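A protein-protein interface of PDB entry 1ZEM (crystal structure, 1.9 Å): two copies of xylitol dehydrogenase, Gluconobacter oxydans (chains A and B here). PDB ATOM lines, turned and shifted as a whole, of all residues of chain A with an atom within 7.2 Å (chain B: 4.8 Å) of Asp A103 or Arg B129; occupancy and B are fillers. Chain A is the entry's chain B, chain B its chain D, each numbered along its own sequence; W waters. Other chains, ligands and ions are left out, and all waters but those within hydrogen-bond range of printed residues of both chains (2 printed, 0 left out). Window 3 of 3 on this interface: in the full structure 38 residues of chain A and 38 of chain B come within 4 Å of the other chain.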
ATOM      1  N   PHE A  98      35.305  23.031 -13.168  1.00  0.00           N
ATOM      2  CA  PHE A  98      35.328  22.165 -11.992  1.00  0.00           C
ATOM      3  C   PHE A  98      34.227  22.645 -11.043  1.00  0.00           C
ATOM      4  O   PHE A  98      34.314  23.739 -10.478  1.00  0.00           O
ATOM      5  CB  PHE A  98      36.642  22.259 -11.256  1.00  0.00           C
ATOM      6  CG  PHE A  98      37.768  21.601 -11.970  1.00  0.00           C
ATOM      7  CD1 PHE A  98      38.352  22.222 -13.080  1.00  0.00           C
ATOM      8  CD2 PHE A  98      38.268  20.363 -11.526  1.00  0.00           C
ATOM      9  CE1 PHE A  98      39.457  21.612 -13.756  1.00  0.00           C
ATOM     10  CE2 PHE A  98      39.375  19.738 -12.197  1.00  0.00           C
ATOM     11  CZ  PHE A  98      39.954  20.366 -13.298  1.00  0.00           C
ATOM     12  N   ALA A  99      33.192  21.836 -10.888  1.00  0.00           N
ATOM     13  CA  ALA A  99      32.090  22.165 -10.013  1.00  0.00           C
ATOM     14  C   ALA A  99      31.400  20.853  -9.774  1.00  0.00           C
ATOM     15  O   ALA A  99      31.501  19.973 -10.603  1.00  0.00           O
ATOM     16  CB  ALA A  99      31.118  23.137 -10.730  1.00  0.00           C
ATOM     17  N   PRO A 100      30.713  20.678  -8.627  1.00  0.00           N
ATOM     18  CA  PRO A 100      29.991  19.426  -8.343  1.00  0.00           C
ATOM     19  C   PRO A 100      28.821  19.391  -9.318  1.00  0.00           C
ATOM     20  O   PRO A 100      28.389  20.423  -9.804  1.00  0.00           O
ATOM     21  CB  PRO A 100      29.561  19.574  -6.882  1.00  0.00           C
ATOM     22  CG  PRO A 100      29.434  21.057  -6.716  1.00  0.00           C
ATOM     23  CD  PRO A 100      30.631  21.611  -7.498  1.00  0.00           C
ATOM     24  N   VAL A 101      28.297  18.202  -9.593  1.00  0.00           N
ATOM     25  CA  VAL A 101      27.311  18.059 -10.629  1.00  0.00           C
ATOM     26  C   VAL A 101      26.065  18.934 -10.534  1.00  0.00           C
ATOM     27  O   VAL A 101      25.589  19.448 -11.568  1.00  0.00           O
ATOM     28  CB  VAL A 101      26.938  16.573 -10.777  1.00  0.00           C
ATOM     29  CG1 VAL A 101      26.247  16.087  -9.510  1.00  0.00           C
ATOM     30  CG2 VAL A 101      26.099  16.339 -12.052  1.00  0.00           C
ATOM     31  N   GLN A 102      25.526  19.090  -9.324  1.00  0.00           N
ATOM     32  CA  GLN A 102      24.323  19.937  -9.138  1.00  0.00           C
ATOM     33  C   GLN A 102      24.517  21.418  -9.562  1.00  0.00           C
ATOM     34  O   GLN A 102      23.536  22.153  -9.789  1.00  0.00           O
ATOM     35  CB  GLN A 102      23.869  19.873  -7.675  1.00  0.00           C
ATOM     36  CG  GLN A 102      24.807  20.571  -6.675  1.00  0.00           C
ATOM     37  CD  GLN A 102      25.911  19.661  -6.117  1.00  0.00           C
ATOM     38  OE1 GLN A 102      26.299  18.684  -6.744  1.00  0.00           O
ATOM     39  NE2 GLN A 102      26.425  20.007  -4.940  1.00  0.00           N
ATOM     40  N   ASP A 103      25.765  21.866  -9.662  1.00  0.00           N
ATOM     41  CA  ASP A 103      26.051  23.244 -10.045  1.00  0.00           C
ATOM     42  C   ASP A 103      26.930  23.328 -11.309  1.00  0.00           C
ATOM     43  O   ASP A 103      27.496  24.373 -11.597  1.00  0.00           O
ATOM     44  CB  ASP A 103      26.841  23.963  -8.948  1.00  0.00           C
ATOM     45  CG  ASP A 103      26.100  24.064  -7.643  1.00  0.00           C
ATOM     46  OD1 ASP A 103      26.778  24.025  -6.606  1.00  0.00           O
ATOM     47  OD2 ASP A 103      24.869  24.192  -7.634  1.00  0.00           O
ATOM     48  N   TYR A 104      27.044  22.235 -12.049  1.00  0.00           N
ATOM     49  CA  TYR A 104      27.928  22.228 -13.195  1.00  0.00           C
ATOM     50  C   TYR A 104      27.349  23.042 -14.321  1.00  0.00           C
ATOM     51  O   TYR A 104      26.232  22.786 -14.748  1.00  0.00           O
ATOM     52  CB  TYR A 104      28.139  20.812 -13.652  1.00  0.00           C
ATOM     53  CG  TYR A 104      29.320  20.741 -14.529  1.00  0.00           C
ATOM     54  CD1 TYR A 104      30.580  20.383 -14.020  1.00  0.00           C
ATOM     55  CD2 TYR A 104      29.204  21.082 -15.874  1.00  0.00           C
ATOM     56  CE1 TYR A 104      31.721  20.367 -14.867  1.00  0.00           C
ATOM     57  CE2 TYR A 104      30.299  21.089 -16.696  1.00  0.00           C
ATOM     58  CZ  TYR A 104      31.544  20.741 -16.206  1.00  0.00           C
ATOM     59  OH  TYR A 104      32.616  20.841 -17.052  1.00  0.00           O
ATOM     60  N   PRO A 105      28.108  24.014 -14.831  1.00  0.00           N
ATOM     61  CA  PRO A 105      27.658  24.889 -15.925  1.00  0.00           C
ATOM     62  C   PRO A 105      27.191  24.069 -17.117  1.00  0.00           C
ATOM     63  O   PRO A 105      27.973  23.333 -17.781  1.00  0.00           O
ATOM     64  CB  PRO A 105      28.892  25.715 -16.262  1.00  0.00           C
ATOM     65  CG  PRO A 105      29.776  25.592 -15.068  1.00  0.00           C
ATOM     66  CD  PRO A 105      29.536  24.213 -14.538  1.00  0.00           C
ATOM     67  N   SER A 106      25.922  24.191 -17.419  1.00  0.00           N
ATOM     68  CA  SER A 106      25.380  23.394 -18.497  1.00  0.00           C
ATOM     69  C   SER A 106      25.950  23.674 -19.891  1.00  0.00           C
ATOM     70  O   SER A 106      26.108  22.754 -20.703  1.00  0.00           O
ATOM     71  CB  SER A 106      23.869  23.526 -18.490  1.00  0.00           C
ATOM     72  OG  SER A 106      23.370  23.011 -17.277  1.00  0.00           O
ATOM     73  N   LYS B 125      21.035  17.000 -13.085  1.00  0.00           N
ATOM     74  CA  LYS B 125      21.372  18.253 -12.398  1.00  0.00           C
ATOM     75  C   LYS B 125      20.174  18.877 -11.677  1.00  0.00           C
ATOM     76  O   LYS B 125      20.269  19.272 -10.472  1.00  0.00           O
ATOM     77  CB  LYS B 125      21.915  19.288 -13.405  1.00  0.00           C
ATOM     78  CG  LYS B 125      22.309  20.643 -12.781  1.00  0.00           C
ATOM     79  CD  LYS B 125      22.867  21.605 -13.829  1.00  0.00           C
ATOM     80  CE  LYS B 125      23.429  22.855 -13.152  1.00  0.00           C
ATOM     81  NZ  LYS B 125      23.612  23.964 -14.115  1.00  0.00           N
ATOM     82  N   ALA B 126      19.073  18.997 -12.413  1.00  0.00           N
ATOM     83  CA  ALA B 126      17.900  19.661 -11.848  1.00  0.00           C
ATOM     84  C   ALA B 126      17.303  18.845 -10.719  1.00  0.00           C
ATOM     85  O   ALA B 126      16.939  19.376  -9.646  1.00  0.00           O
ATOM     86  CB  ALA B 126      16.884  19.904 -12.916  1.00  0.00           C
ATOM     87  N   VAL B 127      17.209  17.545 -10.938  1.00  0.00           N
ATOM     88  CA  VAL B 127      16.666  16.683  -9.904  1.00  0.00           C
ATOM     89  C   VAL B 127      17.589  16.610  -8.683  1.00  0.00           C
ATOM     90  O   VAL B 127      17.104  16.678  -7.542  1.00  0.00           O
ATOM     91  CB  VAL B 127      16.391  15.310 -10.481  1.00  0.00           C
ATOM     92  CG1 VAL B 127      15.914  14.339  -9.384  1.00  0.00           C
ATOM     93  CG2 VAL B 127      15.355  15.466 -11.597  1.00  0.00           C
ATOM     94  N   SER B 128      18.897  16.517  -8.904  1.00  0.00           N
ATOM     95  CA  SER B 128      19.843  16.431  -7.808  1.00  0.00           C
ATOM     96  C   SER B 128      19.782  17.639  -6.867  1.00  0.00           C
ATOM     97  O   SER B 128      19.922  17.481  -5.649  1.00  0.00           O
ATOM     98  CB  SER B 128      21.279  16.220  -8.313  1.00  0.00           C
ATOM     99  OG  SER B 128      21.802  17.395  -8.898  1.00  0.00           O
ATOM    100  N   ARG B 129      19.555  18.821  -7.412  1.00  0.00           N
ATOM    101  CA  ARG B 129      19.414  20.039  -6.576  1.00  0.00           C
ATOM    102  C   ARG B 129      18.216  19.886  -5.645  1.00  0.00           C
ATOM    103  O   ARG B 129      18.227  20.326  -4.481  1.00  0.00           O
ATOM    104  CB  ARG B 129      19.159  21.256  -7.464  1.00  0.00           C
ATOM    105  CG  ARG B 129      20.374  21.679  -8.270  1.00  0.00           C
ATOM    106  CD  ARG B 129      20.034  22.838  -9.166  1.00  0.00           C
ATOM    107  NE  ARG B 129      21.252  23.544  -9.496  1.00  0.00           N
ATOM    108  CZ  ARG B 129      21.317  24.644 -10.228  1.00  0.00           C
ATOM    109  NH1 ARG B 129      20.201  25.190 -10.733  1.00  0.00           N
ATOM    110  NH2 ARG B 129      22.504  25.202 -10.436  1.00  0.00           N
ATOM    111  N   GLN B 130      17.150  19.318  -6.171  1.00  0.00           N
ATOM    112  CA  GLN B 130      15.974  19.125  -5.344  1.00  0.00           C
ATOM    113  C   GLN B 130      16.306  18.089  -4.276  1.00  0.00           C
ATOM    114  O   GLN B 130      16.014  18.275  -3.112  1.00  0.00           O
ATOM    115  CB  GLN B 130      14.781  18.626  -6.179  1.00  0.00           C
ATOM    116  CG  GLN B 130      13.583  18.092  -5.375  1.00  0.00           C
ATOM    117  CD  GLN B 130      12.841  19.201  -4.610  1.00  0.00           C
ATOM    118  OE1 GLN B 130      12.891  20.367  -5.007  1.00  0.00           O
ATOM    119  NE2 GLN B 130      12.160  18.837  -3.516  1.00  0.00           N
ATOM    120  N   MET B 131      16.954  16.994  -4.668  1.00  0.00           N
ATOM    121  CA  MET B 131      17.267  15.971  -3.683  1.00  0.00           C
ATOM    122  C   MET B 131      18.156  16.519  -2.631  1.00  0.00           C
ATOM    123  O   MET B 131      18.075  16.096  -1.493  1.00  0.00           O
ATOM    124  CB  MET B 131      17.904  14.737  -4.335  1.00  0.00           C
ATOM    125  CG  MET B 131      16.919  13.964  -5.185  1.00  0.00           C
ATOM    126  SD  MET B 131      17.820  12.737  -6.214  1.00  0.00           S
ATOM    127  CE  MET B 131      16.476  11.705  -6.712  1.00  0.00           C
ATOM    128  N   ILE B 132      19.003  17.474  -2.987  1.00  0.00           N
ATOM    129  CA  ILE B 132      19.892  18.067  -2.017  1.00  0.00           C
ATOM    130  C   ILE B 132      19.062  18.807  -0.952  1.00  0.00           C
ATOM    131  O   ILE B 132      19.309  18.658   0.240  1.00  0.00           O
ATOM    132  CB  ILE B 132      20.863  18.998  -2.711  1.00  0.00           C
ATOM    133  CG1 ILE B 132      21.878  18.135  -3.516  1.00  0.00           C
ATOM    134  CG2 ILE B 132      21.603  19.853  -1.690  1.00  0.00           C
ATOM    135  CD1 ILE B 132      22.940  18.921  -4.283  1.00  0.00           C
ATOM    136  N   THR B 133      18.051  19.560  -1.377  1.00  0.00           N
ATOM    137  CA  THR B 133      17.191  20.275  -0.404  1.00  0.00           C
ATOM    138  C   THR B 133      16.455  19.283   0.486  1.00  0.00           C
ATOM    139  O   THR B 133      16.075  19.636   1.611  1.00  0.00           O
ATOM    140  CB  THR B 133      16.102  21.140  -1.068  1.00  0.00           C
ATOM    141  OG1 THR B 133      15.063  20.287  -1.579  1.00  0.00           O
ATOM    142  CG2 THR B 133      16.685  21.973  -2.156  1.00  0.00           C
HETATM  143  O   HOH W   1      25.058  25.944 -12.654  1.00  0.00           O
HETATM  144  O   HOH W   2      24.226  26.006 -15.983  1.00  0.00           O
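No position is printed for both chains.
Of the 9 pairs that touch across the chains among the printed residues, none has its exchanged pair printed and touching as well.
CG of Lys B125 touches O of Val A101 (3.7 Å).
Lys B125 touches Gln A102.
Gln A102 touches Ser B128.
Gln A102 touches Ile B132.
C of Asp A103 touches CE of Lys B125 (3.98 Å).
Of the printed residues of chain B, Val A101 touches Lys B125 (3.7 Å).
Of the printed residues of chain B, Asp A103 touches Lys B125 (3.98 Å) and Arg B129 (3.8 Å).
Of the printed residues of chain B, Tyr A104 touches Lys B125.
Printed residues of chain B within 4 Å of Ser A106: Lys B125.
Ala B126 touches none of the printed residues of chain A.
Of chain A, only Gln A102 and Asp A103 come within 4 Å of Arg B129.
Gln B130 touches none of the printed residues of chain A.
Of the printed residues of chain A, Ile B132 touches Gln A102 (3.5 Å).
The nearest printed residue of chain B that does not touch Asp A103 is Ser B128 (6.0 Å).
The nearest residue of chain A that does not touch Arg B129 is Tyr A104 (5.7 Å).
Water W2 lies within hydrogen-bond range of NZ of Lys B125 and N of Ser A106.
Water W1 lies within hydrogen-bond range of the side-chain amino group (NZ) of Lys B125 (2.9 Å), the backbone carbonyl oxygen (O) of Asp A103 (3.1 Å) and the guanidinium group (NH2) of Arg B129 (3.5 Å).
The backbone carbonyl oxygen (O) of Lys B125 is in hydrogen-bond range of the side-chain hydroxyl (OG) of Ser B128, at 2.9 Å.
The backbone carbonyl oxygen (O) of Gln A102 is in hydrogen-bond range of the guanidinium group (NE) of Arg B129 (2.7 Å).
The side-chain carboxylate (OD2) of Asp A103 is in salt-bridge range of the guanidinium group (NH2) of Arg B129 (3.8 Å).
O of Tyr A104 sits at hydrogen-bond distance from NZ of Lys B125.
The side-chain hydroxyl of Ser A106 lies within hydrogen-bond range of the side-chain amino group of Lys B125 (3.3 Å).
Printed residues of chain A that touch a printed residue of chain B: Val A101, Gln A102, Asp A103, Tyr A104 and Ser A106.
Hydrophobic or aromatic side chains of chain B that line the printed part of chain A: Ile B132.
Among the printed residues, 9 pairs touch across the chains.
Among the printed residues, Asp or Glu carboxylates within 4 Å of a Lys or Arg side-chain nitrogen of the other chain: Asp A103 with Arg B129.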
